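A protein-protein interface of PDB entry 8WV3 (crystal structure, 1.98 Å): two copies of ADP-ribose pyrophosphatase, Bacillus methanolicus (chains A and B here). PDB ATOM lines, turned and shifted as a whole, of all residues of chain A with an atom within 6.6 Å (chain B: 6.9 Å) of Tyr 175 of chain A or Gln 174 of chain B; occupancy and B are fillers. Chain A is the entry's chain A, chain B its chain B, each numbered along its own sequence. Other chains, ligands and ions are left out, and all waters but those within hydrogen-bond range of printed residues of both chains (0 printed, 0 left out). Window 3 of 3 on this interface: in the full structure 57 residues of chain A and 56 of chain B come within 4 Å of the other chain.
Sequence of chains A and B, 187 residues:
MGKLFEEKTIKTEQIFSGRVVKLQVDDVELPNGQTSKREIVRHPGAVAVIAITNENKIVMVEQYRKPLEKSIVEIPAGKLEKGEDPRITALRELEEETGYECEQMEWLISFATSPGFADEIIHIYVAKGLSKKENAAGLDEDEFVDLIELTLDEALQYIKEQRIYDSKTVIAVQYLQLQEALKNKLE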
ATOM      1  N   ILE A  50      21.722 -12.522 -18.633  1.00  0.00           N
ATOM      2  CA  ILE A  50      20.733 -13.393 -18.009  1.00  0.00           C
ATOM      3  C   ILE A  50      19.967 -14.050 -19.154  1.00  0.00           C
ATOM      4  O   ILE A  50      19.223 -13.380 -19.872  1.00  0.00           O
ATOM      5  CB  ILE A  50      19.778 -12.617 -17.096  1.00  0.00           C
ATOM      6  CG1 ILE A  50      20.566 -11.903 -15.975  1.00  0.00           C
ATOM      7  CG2 ILE A  50      18.710 -13.571 -16.500  1.00  0.00           C
ATOM      8  CD1 ILE A  50      19.670 -11.055 -15.080  1.00  0.00           C
ATOM      9  N   LEU A 108      19.333  -4.393 -18.847  1.00  0.00           N
ATOM     10  CA  LEU A 108      18.601  -4.399 -17.591  1.00  0.00           C
ATOM     11  C   LEU A 108      19.125  -3.376 -16.591  1.00  0.00           C
ATOM     12  O   LEU A 108      18.354  -2.552 -16.081  1.00  0.00           O
ATOM     13  CB  LEU A 108      18.650  -5.809 -16.975  1.00  0.00           C
ATOM     14  CG  LEU A 108      18.019  -5.955 -15.603  1.00  0.00           C
ATOM     15  CD1 LEU A 108      16.534  -5.664 -15.685  1.00  0.00           C
ATOM     16  CD2 LEU A 108      18.267  -7.357 -15.104  1.00  0.00           C
ATOM     17  N   ILE A 109      20.433  -3.373 -16.330  1.00  0.00           N
ATOM     18  CA  ILE A 109      21.005  -2.557 -15.242  1.00  0.00           C
ATOM     19  C   ILE A 109      22.516  -2.518 -15.398  1.00  0.00           C
ATOM     20  O   ILE A 109      23.116  -3.468 -15.935  1.00  0.00           O
ATOM     21  CB  ILE A 109      20.610  -3.114 -13.855  1.00  0.00           C
ATOM     22  CG1 ILE A 109      20.988  -2.133 -12.729  1.00  0.00           C
ATOM     23  CG2 ILE A 109      21.289  -4.481 -13.587  1.00  0.00           C
ATOM     24  CD1 ILE A 109      20.334  -2.483 -11.390  1.00  0.00           C
ATOM     25  N   VAL A 126      19.349  -9.024 -20.617  1.00  0.00           N
ATOM     26  CA  VAL A 126      18.463 -10.180 -20.481  1.00  0.00           C
ATOM     27  C   VAL A 126      18.182 -10.723 -21.883  1.00  0.00           C
ATOM     28  O   VAL A 126      17.708  -9.989 -22.753  1.00  0.00           O
ATOM     29  CB  VAL A 126      17.160  -9.823 -19.746  1.00  0.00           C
ATOM     30  CG1 VAL A 126      16.223 -11.035 -19.718  1.00  0.00           C
ATOM     31  CG2 VAL A 126      17.447  -9.381 -18.314  1.00  0.00           C
ATOM     32  N   SER A 167      28.896 -10.779  -7.280  1.00  0.00           N
ATOM     33  CA  SER A 167      27.788  -9.820  -7.204  1.00  0.00           C
ATOM     34  C   SER A 167      26.881  -9.899  -8.437  1.00  0.00           C
ATOM     35  O   SER A 167      25.652  -9.820  -8.315  1.00  0.00           O
ATOM     36  CB  SER A 167      28.316  -8.397  -6.997  1.00  0.00           C
ATOM     37  OG  SER A 167      29.360  -8.069  -7.885  1.00  0.00           O
ATOM     38  N   VAL A 170      24.518 -12.952  -8.138  1.00  0.00           N
ATOM     39  CA  VAL A 170      23.514 -12.782  -7.098  1.00  0.00           C
ATOM     40  C   VAL A 170      22.445 -11.814  -7.576  1.00  0.00           C
ATOM     41  O   VAL A 170      21.251 -12.010  -7.329  1.00  0.00           O
ATOM     42  CB  VAL A 170      24.170 -12.294  -5.786  1.00  0.00           C
ATOM     43  CG1 VAL A 170      23.107 -11.820  -4.815  1.00  0.00           C
ATOM     44  CG2 VAL A 170      24.961 -13.409  -5.169  1.00  0.00           C
ATOM     45  N   ILE A 171      22.864 -10.723  -8.215  1.00  0.00           N
ATOM     46  CA  ILE A 171      21.908  -9.755  -8.748  1.00  0.00           C
ATOM     47  C   ILE A 171      20.979 -10.428  -9.757  1.00  0.00           C
ATOM     48  O   ILE A 171      19.764 -10.185  -9.770  1.00  0.00           O
ATOM     49  CB  ILE A 171      22.666  -8.559  -9.372  1.00  0.00           C
ATOM     50  CG1 ILE A 171      23.261  -7.682  -8.268  1.00  0.00           C
ATOM     51  CG2 ILE A 171      21.743  -7.729 -10.272  1.00  0.00           C
ATOM     52  CD1 ILE A 171      24.279  -6.649  -8.788  1.00  0.00           C
ATOM     53  N   ALA A 172      21.529 -11.306 -10.594  1.00  0.00           N
ATOM     54  CA  ALA A 172      20.710 -12.021 -11.582  1.00  0.00           C
ATOM     55  C   ALA A 172      19.695 -12.947 -10.911  1.00  0.00           C
ATOM     56  O   ALA A 172      18.538 -13.027 -11.344  1.00  0.00           O
ATOM     57  CB  ALA A 172      21.623 -12.824 -12.528  1.00  0.00           C
ATOM     58  N   VAL A 173      20.114 -13.687  -9.877  1.00  0.00           N
ATOM     59  CA  VAL A 173      19.180 -14.594  -9.202  1.00  0.00           C
ATOM     60  C   VAL A 173      18.061 -13.805  -8.529  1.00  0.00           C
ATOM     61  O   VAL A 173      16.887 -14.165  -8.626  1.00  0.00           O
ATOM     62  CB  VAL A 173      19.916 -15.489  -8.183  1.00  0.00           C
ATOM     63  CG1 VAL A 173      18.909 -16.339  -7.375  1.00  0.00           C
ATOM     64  CG2 VAL A 173      20.904 -16.372  -8.876  1.00  0.00           C
ATOM     65  N   GLN A 174      18.406 -12.717  -7.823  1.00  0.00           N
ATOM     66  CA  GLN A 174      17.361 -11.908  -7.195  1.00  0.00           C
ATOM     67  C   GLN A 174      16.433 -11.286  -8.228  1.00  0.00           C
ATOM     68  O   GLN A 174      15.216 -11.216  -8.021  1.00  0.00           O
ATOM     69  CB  GLN A 174      17.984 -10.852  -6.286  1.00  0.00           C
ATOM     70  CG  GLN A 174      18.773 -11.532  -5.222  1.00  0.00           C
ATOM     71  CD  GLN A 174      19.020 -10.661  -4.033  1.00  0.00           C
ATOM     72  OE1 GLN A 174      18.874 -11.118  -2.889  1.00  0.00           O
ATOM     73  NE2 GLN A 174      19.397  -9.401  -4.279  1.00  0.00           N
ATOM     74  N   TYR A 175      16.972 -10.898  -9.374  1.00  0.00           N
ATOM     75  CA  TYR A 175      16.130 -10.427 -10.463  1.00  0.00           C
ATOM     76  C   TYR A 175      15.088 -11.467 -10.853  1.00  0.00           C
ATOM     77  O   TYR A 175      13.900 -11.150 -11.010  1.00  0.00           O
ATOM     78  CB  TYR A 175      16.988 -10.092 -11.672  1.00  0.00           C
ATOM     79  CG  TYR A 175      16.147  -9.686 -12.842  1.00  0.00           C
ATOM     80  CD1 TYR A 175      15.489  -8.465 -12.841  1.00  0.00           C
ATOM     81  CD2 TYR A 175      15.946 -10.549 -13.908  1.00  0.00           C
ATOM     82  CE1 TYR A 175      14.702  -8.086 -13.895  1.00  0.00           C
ATOM     83  CE2 TYR A 175      15.155 -10.175 -14.981  1.00  0.00           C
ATOM     84  CZ  TYR A 175      14.531  -8.943 -14.962  1.00  0.00           C
ATOM     85  OH  TYR A 175      13.740  -8.531 -16.010  1.00  0.00           O
ATOM     86  N   LEU A 176      15.528 -12.712 -11.051  1.00  0.00           N
ATOM     87  CA  LEU A 176      14.605 -13.779 -11.420  1.00  0.00           C
ATOM     88  C   LEU A 176      13.622 -14.080 -10.293  1.00  0.00           C
ATOM     89  O   LEU A 176      12.445 -14.339 -10.553  1.00  0.00           O
ATOM     90  CB  LEU A 176      15.394 -15.030 -11.825  1.00  0.00           C
ATOM     91  CG  LEU A 176      16.292 -14.767 -13.039  1.00  0.00           C
ATOM     92  CD1 LEU A 176      17.031 -16.016 -13.495  1.00  0.00           C
ATOM     93  CD2 LEU A 176      15.437 -14.227 -14.183  1.00  0.00           C
ATOM     94  N   GLN A 177      14.079 -14.049  -9.034  1.00  0.00           N
ATOM     95  CA  GLN A 177      13.152 -14.157  -7.912  1.00  0.00           C
ATOM     96  C   GLN A 177      12.074 -13.093  -8.000  1.00  0.00           C
ATOM     97  O   GLN A 177      10.897 -13.358  -7.743  1.00  0.00           O
ATOM     98  CB  GLN A 177      13.893 -13.979  -6.603  1.00  0.00           C
ATOM     99  CG  GLN A 177      14.520 -15.188  -6.036  1.00  0.00           C
ATOM    100  CD  GLN A 177      15.203 -14.839  -4.742  1.00  0.00           C
ATOM    101  OE1 GLN A 177      16.313 -14.320  -4.762  1.00  0.00           O
ATOM    102  NE2 GLN A 177      14.549 -15.102  -3.619  1.00  0.00           N
ATOM    103  N   LEU A 178      12.469 -11.869  -8.335  1.00  0.00           N
ATOM    104  CA  LEU A 178      11.511 -10.783  -8.465  1.00  0.00           C
ATOM    105  C   LEU A 178      10.512 -11.052  -9.588  1.00  0.00           C
ATOM    106  O   LEU A 178       9.307 -10.876  -9.402  1.00  0.00           O
ATOM    107  CB  LEU A 178      12.260  -9.465  -8.689  1.00  0.00           C
ATOM    108  CG  LEU A 178      12.679  -8.917  -7.327  1.00  0.00           C
ATOM    109  CD1 LEU A 178      13.753  -7.806  -7.393  1.00  0.00           C
ATOM    110  CD2 LEU A 178      11.431  -8.469  -6.570  1.00  0.00           C
ATOM    111  N   GLN A 179      10.983 -11.484 -10.755  1.00  0.00           N
ATOM    112  CA  GLN A 179      10.054 -11.766 -11.850  1.00  0.00           C
ATOM    113  C   GLN A 179       8.989 -12.761 -11.413  1.00  0.00           C
ATOM    114  O   GLN A 179       7.822 -12.654 -11.811  1.00  0.00           O
ATOM    115  CB  GLN A 179      10.817 -12.283 -13.072  1.00  0.00           C
ATOM    116  CG  GLN A 179      11.670 -11.219 -13.722  1.00  0.00           C
ATOM    117  CD  GLN A 179      10.897  -9.922 -13.947  1.00  0.00           C
ATOM    118  OE1 GLN A 179      11.221  -8.875 -13.382  1.00  0.00           O
ATOM    119  NE2 GLN A 179       9.884  -9.987 -14.804  1.00  0.00           N
ATOM    120  N   GLU A 180       9.371 -13.709 -10.557  1.00  0.00           N
ATOM    121  CA  GLU A 180       8.450 -14.733 -10.078  1.00  0.00           C
ATOM    122  C   GLU A 180       7.424 -14.150  -9.116  1.00  0.00           C
ATOM    123  O   GLU A 180       6.222 -14.401  -9.249  1.00  0.00           O
ATOM    124  CB  GLU A 180       9.237 -15.854  -9.408  1.00  0.00           C
ATOM    125  CG  GLU A 180       9.876 -16.783 -10.408  1.00  0.00           C
ATOM    126  CD  GLU A 180       8.937 -17.115 -11.545  1.00  0.00           C
ATOM    127  OE1 GLU A 180       8.036 -17.956 -11.329  1.00  0.00           O
ATOM    128  OE2 GLU A 180       9.079 -16.515 -12.639  1.00  0.00           O
ATOM    129  N   LEU B 152      11.557   2.328  -0.303  1.00  0.00           N
ATOM    130  CA  LEU B 152      11.847   1.396  -1.389  1.00  0.00           C
ATOM    131  C   LEU B 152      11.661   2.073  -2.743  1.00  0.00           C
ATOM    132  O   LEU B 152      12.540   2.005  -3.611  1.00  0.00           O
ATOM    133  CB  LEU B 152      10.968   0.155  -1.270  1.00  0.00           C
ATOM    134  CG  LEU B 152      11.083  -0.814  -2.443  1.00  0.00           C
ATOM    135  CD1 LEU B 152      12.528  -1.280  -2.607  1.00  0.00           C
ATOM    136  CD2 LEU B 152      10.119  -2.003  -2.278  1.00  0.00           C
ATOM    137  N   LEU B 156      14.432   2.604  -5.652  1.00  0.00           N
ATOM    138  CA  LEU B 156      14.307   2.136  -7.032  1.00  0.00           C
ATOM    139  C   LEU B 156      14.461   3.290  -8.015  1.00  0.00           C
ATOM    140  O   LEU B 156      15.052   3.125  -9.089  1.00  0.00           O
ATOM    141  CB  LEU B 156      12.968   1.419  -7.223  1.00  0.00           C
ATOM    142  CG  LEU B 156      12.843   0.025  -6.598  1.00  0.00           C
ATOM    143  CD1 LEU B 156      11.367  -0.345  -6.459  1.00  0.00           C
ATOM    144  CD2 LEU B 156      13.559  -1.046  -7.428  1.00  0.00           C
ATOM    145  N   ILE B 159      18.087   3.919  -8.427  1.00  0.00           N
ATOM    146  CA  ILE B 159      18.721   2.968  -9.350  1.00  0.00           C
ATOM    147  C   ILE B 159      18.473   3.390 -10.794  1.00  0.00           C
ATOM    148  O   ILE B 159      19.376   3.366 -11.637  1.00  0.00           O
ATOM    149  CB  ILE B 159      18.206   1.545  -9.096  1.00  0.00           C
ATOM    150  CG1 ILE B 159      18.753   0.995  -7.778  1.00  0.00           C
ATOM    151  CG2 ILE B 159      18.558   0.619 -10.305  1.00  0.00           C
ATOM    152  CD1 ILE B 159      18.312  -0.462  -7.524  1.00  0.00           C
ATOM    153  N   SER B 167      27.496  -2.893  -6.632  1.00  0.00           N
ATOM    154  CA  SER B 167      26.814  -4.183  -6.579  1.00  0.00           C
ATOM    155  C   SER B 167      26.164  -4.420  -5.227  1.00  0.00           C
ATOM    156  O   SER B 167      25.021  -4.894  -5.164  1.00  0.00           O
ATOM    157  CB  SER B 167      27.783  -5.315  -6.944  1.00  0.00           C
ATOM    158  OG  SER B 167      29.002  -5.154  -6.270  1.00  0.00           O
ATOM    159  N   THR B 169      24.919  -2.349  -2.988  1.00  0.00           N
ATOM    160  CA  THR B 169      23.695  -1.590  -2.756  1.00  0.00           C
ATOM    161  C   THR B 169      22.553  -2.044  -3.668  1.00  0.00           C
ATOM    162  O   THR B 169      21.386  -2.045  -3.247  1.00  0.00           O
ATOM    163  CB  THR B 169      23.989  -0.098  -2.926  1.00  0.00           C
ATOM    164  OG1 THR B 169      25.170   0.213  -2.168  1.00  0.00           O
ATOM    165  CG2 THR B 169      22.775   0.753  -2.427  1.00  0.00           C
ATOM    166  N   VAL B 170      22.849  -2.435  -4.904  1.00  0.00           N
ATOM    167  CA  VAL B 170      21.795  -3.015  -5.746  1.00  0.00           C
ATOM    168  C   VAL B 170      21.232  -4.258  -5.080  1.00  0.00           C
ATOM    169  O   VAL B 170      20.014  -4.439  -4.998  1.00  0.00           O
ATOM    170  CB  VAL B 170      22.322  -3.326  -7.157  1.00  0.00           C
ATOM    171  CG1 VAL B 170      21.316  -4.166  -7.954  1.00  0.00           C
ATOM    172  CG2 VAL B 170      22.636  -2.027  -7.910  1.00  0.00           C
ATOM    173  N   ILE B 171      22.115  -5.114  -4.557  1.00  0.00           N
ATOM    174  CA  ILE B 171      21.651  -6.339  -3.893  1.00  0.00           C
ATOM    175  C   ILE B 171      20.765  -6.006  -2.699  1.00  0.00           C
ATOM    176  O   ILE B 171      19.748  -6.672  -2.459  1.00  0.00           O
ATOM    177  CB  ILE B 171      22.860  -7.211  -3.494  1.00  0.00           C
ATOM    178  CG1 ILE B 171      23.518  -7.737  -4.779  1.00  0.00           C
ATOM    179  CG2 ILE B 171      22.443  -8.343  -2.505  1.00  0.00           C
ATOM    180  CD1 ILE B 171      24.907  -8.346  -4.635  1.00  0.00           C
ATOM    181  N   ALA B 172      21.134  -4.969  -1.933  1.00  0.00           N
ATOM    182  CA  ALA B 172      20.317  -4.539  -0.801  1.00  0.00           C
ATOM    183  C   ALA B 172      18.931  -4.083  -1.244  1.00  0.00           C
ATOM    184  O   ALA B 172      17.914  -4.469  -0.643  1.00  0.00           O
ATOM    185  CB  ALA B 172      21.026  -3.412  -0.032  1.00  0.00           C
ATOM    186  N   VAL B 173      18.862  -3.240  -2.279  1.00  0.00           N
ATOM    187  CA  VAL B 173      17.556  -2.797  -2.761  1.00  0.00           C
ATOM    188  C   VAL B 173      16.723  -3.991  -3.214  1.00  0.00           C
ATOM    189  O   VAL B 173      15.526  -4.099  -2.901  1.00  0.00           O
ATOM    190  CB  VAL B 173      17.721  -1.748  -3.878  1.00  0.00           C
ATOM    191  CG1 VAL B 173      16.363  -1.357  -4.446  1.00  0.00           C
ATOM    192  CG2 VAL B 173      18.452  -0.493  -3.330  1.00  0.00           C
ATOM    193  N   GLN B 174      17.339  -4.915  -3.947  1.00  0.00           N
ATOM    194  CA  GLN B 174      16.616  -6.111  -4.376  1.00  0.00           C
ATOM    195  C   GLN B 174      16.057  -6.866  -3.185  1.00  0.00           C
ATOM    196  O   GLN B 174      14.979  -7.468  -3.262  1.00  0.00           O
ATOM    197  CB  GLN B 174      17.553  -7.028  -5.159  1.00  0.00           C
ATOM    198  CG  GLN B 174      17.861  -6.569  -6.548  1.00  0.00           C
ATOM    199  CD  GLN B 174      18.763  -7.577  -7.226  1.00  0.00           C
ATOM    200  OE1 GLN B 174      19.682  -8.124  -6.592  1.00  0.00           O
ATOM    201  NE2 GLN B 174      18.462  -7.897  -8.467  1.00  0.00           N
ATOM    202  N   TYR B 175      16.802  -6.875  -2.083  1.00  0.00           N
ATOM    203  CA  TYR B 175      16.390  -7.620  -0.903  1.00  0.00           C
ATOM    204  C   TYR B 175      15.190  -6.948  -0.243  1.00  0.00           C
ATOM    205  O   TYR B 175      14.227  -7.615   0.145  1.00  0.00           O
ATOM    206  CB  TYR B 175      17.582  -7.737   0.062  1.00  0.00           C
ATOM    207  CG  TYR B 175      17.204  -8.157   1.450  1.00  0.00           C
ATOM    208  CD1 TYR B 175      17.086  -9.501   1.793  1.00  0.00           C
ATOM    209  CD2 TYR B 175      16.910  -7.201   2.411  1.00  0.00           C
ATOM    210  CE1 TYR B 175      16.717  -9.881   3.090  1.00  0.00           C
ATOM    211  CE2 TYR B 175      16.538  -7.560   3.685  1.00  0.00           C
ATOM    212  CZ  TYR B 175      16.441  -8.898   4.023  1.00  0.00           C
ATOM    213  OH  TYR B 175      16.064  -9.212   5.306  1.00  0.00           O
ATOM    214  N   LEU B 176      15.227  -5.626  -0.122  1.00  0.00           N
ATOM    215  CA  LEU B 176      14.037  -4.896   0.302  1.00  0.00           C
ATOM    216  C   LEU B 176      12.855  -5.175  -0.611  1.00  0.00           C
ATOM    217  O   LEU B 176      11.732  -5.401  -0.140  1.00  0.00           O
ATOM    218  CB  LEU B 176      14.345  -3.407   0.359  1.00  0.00           C
ATOM    219  CG  LEU B 176      15.654  -3.198   1.089  1.00  0.00           C
ATOM    220  CD1 LEU B 176      15.773  -1.803   1.659  1.00  0.00           C
ATOM    221  CD2 LEU B 176      15.658  -4.200   2.238  1.00  0.00           C
ATOM    222  N   GLN B 177      13.093  -5.185  -1.920  1.00  0.00           N
ATOM    223  CA  GLN B 177      12.019  -5.446  -2.869  1.00  0.00           C
ATOM    224  C   GLN B 177      11.362  -6.797  -2.604  1.00  0.00           C
ATOM    225  O   GLN B 177      10.136  -6.929  -2.687  1.00  0.00           O
ATOM    226  CB  GLN B 177      12.583  -5.391  -4.283  1.00  0.00           C
ATOM    227  CG  GLN B 177      12.207  -4.178  -5.059  1.00  0.00           C
ATOM    228  CD  GLN B 177      12.602  -4.297  -6.516  1.00  0.00           C
ATOM    229  OE1 GLN B 177      13.733  -4.676  -6.827  1.00  0.00           O
ATOM    230  NE2 GLN B 177      11.681  -3.976  -7.412  1.00  0.00           N
ATOM    231  N   LEU B 178      12.165  -7.818  -2.290  1.00  0.00           N
ATOM    232  CA  LEU B 178      11.613  -9.144  -2.023  1.00  0.00           C
ATOM    233  C   LEU B 178      10.917  -9.190  -0.669  1.00  0.00           C
ATOM    234  O   LEU B 178       9.892  -9.862  -0.516  1.00  0.00           O
ATOM    235  CB  LEU B 178      12.721 -10.195  -2.102  1.00  0.00           C
ATOM    236  CG  LEU B 178      13.258 -10.512  -3.501  1.00  0.00           C
ATOM    237  CD1 LEU B 178      14.448 -11.456  -3.416  1.00  0.00           C
ATOM    238  CD2 LEU B 178      12.167 -11.134  -4.399  1.00  0.00           C
ATOM    239  N   GLN B 179      11.460  -8.486   0.327  1.00  0.00           N
ATOM    240  CA  GLN B 179      10.808  -8.436   1.629  1.00  0.00           C
ATOM    241  C   GLN B 179       9.439  -7.768   1.538  1.00  0.00           C
ATOM    242  O   GLN B 179       8.473  -8.232   2.152  1.00  0.00           O
ATOM    243  CB  GLN B 179      11.699  -7.706   2.630  1.00  0.00           C
ATOM    244  CG  GLN B 179      12.958  -8.466   3.031  1.00  0.00           C
ATOM    245  CD  GLN B 179      12.675  -9.919   3.343  1.00  0.00           C
ATOM    246  OE1 GLN B 179      13.025 -10.818   2.573  1.00  0.00           O
ATOM    247  NE2 GLN B 179      12.023 -10.157   4.470  1.00  0.00           N
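Of the 15 printed residues of chain B, 7 touch a printed residue of chain A.
Printed residues of chain B that touch a printed residue of chain A: Ile 159, Ser 167, Val 170, Ile 171, Gln 174, Gln 177 and Leu 178.
Hydrophobic or aromatic side chains of chain B within 4 Å of the printed part of chain A: Ile 159, Val 170, Ile 171 and Leu 178.
Of the 16 printed residues of chain A, 8 touch a printed residue of chain B.
Hydrophobic or aromatic side chains of chain A within 4 Å of the printed part of chain B: Ile 109, Val 170, Ile 171 and Leu 178.
Among the printed residues, no Asp or Glu carboxylate lies within 4 Å of a Lys or Arg side-chain nitrogen of the other chain.
Tyr 175 of chain A touches one residue of chain B.
Gln 174 of chain B touches just these residues of chain A: Ile 171, Gln 174 and Tyr 175.
Of the printed residues of chain B, Leu 178 of chain A touches Gln 177 (3.2 Å) and Leu 178 (3.5 Å).
Printed residues of chain A within 4 Å of Ile 171 of chain B: Val 170 (3.9 Å), Ile 171 (3.5 Å) and Gln 174 (3.3 Å).
Of the printed residues of chain B, Ile 109 of chain A touches Ile 159 (3.7 Å) and Val 170 (3.95 Å).
The nearest residue of chain B that does not touch Tyr 175 of chain A is Leu 178 of chain B (6.5 Å).
The nearest residue of chain A that does not touch Gln 174 of chain B is Val 170 of chain A (4.3 Å).
Ser 167 of chain A touches its own counterpart, Ser 167 of chain B.
Val 170 of chain A touches Ile 171 of chain B, and with the chains exchanged Ile 171 of chain A touches Val 170 of chain B.
Gln 174 of chain B touches its own counterpart, Gln 174 of chain A.
Gln 177 of chain A touches Leu 178 of chain B, and with the chains exchanged Leu 178 of chain A touches Gln 177 of chain B.
Positions printed for both chains: 167, 170, 171, 172, 173, 174, 175, 176, 177, 178 and 179.
Of the 13 pairs that touch across the chains among the printed residues, 10 have their exchanged pair printed and touching as well.
NE2 of Gln 174 of chain B lies close to N of Tyr 175 of chain A, 3.5 Å away.
The side-chain hydroxyl of Ser 167 of chain A lies close to the side-chain hydroxyl of Ser 167 of chain B (3.4 Å).
NE2 of Gln 174 of chain A lies within hydrogen-bond range of OE1 of Gln 174 of chain B, at 2.7 Å.
The backbone carbonyl oxygen (O) of Ile 171 of chain B sits at hydrogen-bond distance from the side-chain amide nitrogen (NE2) of Gln 174 of chain A, 3.3 Å away.
The backbone carbonyl oxygen (O) of Ile 171 of chain A sits at hydrogen-bond distance from the side-chain amide nitrogen (NE2) of Gln 174 of chain B (2.9 Å).
Ile 109 of chain A touches Ile 159 of chain B (CD1 to CG2, 3.7 Å).
CD1 of Ile 109 of chain A touches CG1 of Val 170 of chain B, at 3.95 Å.
CD1 of Ile 171 of chain B touches CG1 of Val 170 of chain A, 3.9 Å away.
Ile 171 of chain A touches Val 170 of chain B.
Ile 171 of chain A touches Ile 171 of chain B.
Gln 177 of chain A touches Leu 178 of chain B (NE2 to CD1, 3.7 Å).
Gln 177 of chain B touches Leu 178 of chain A (OE1 to CD1, 3.2 Å).
Leu 178 of chain A touches Leu 178 of chain B.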
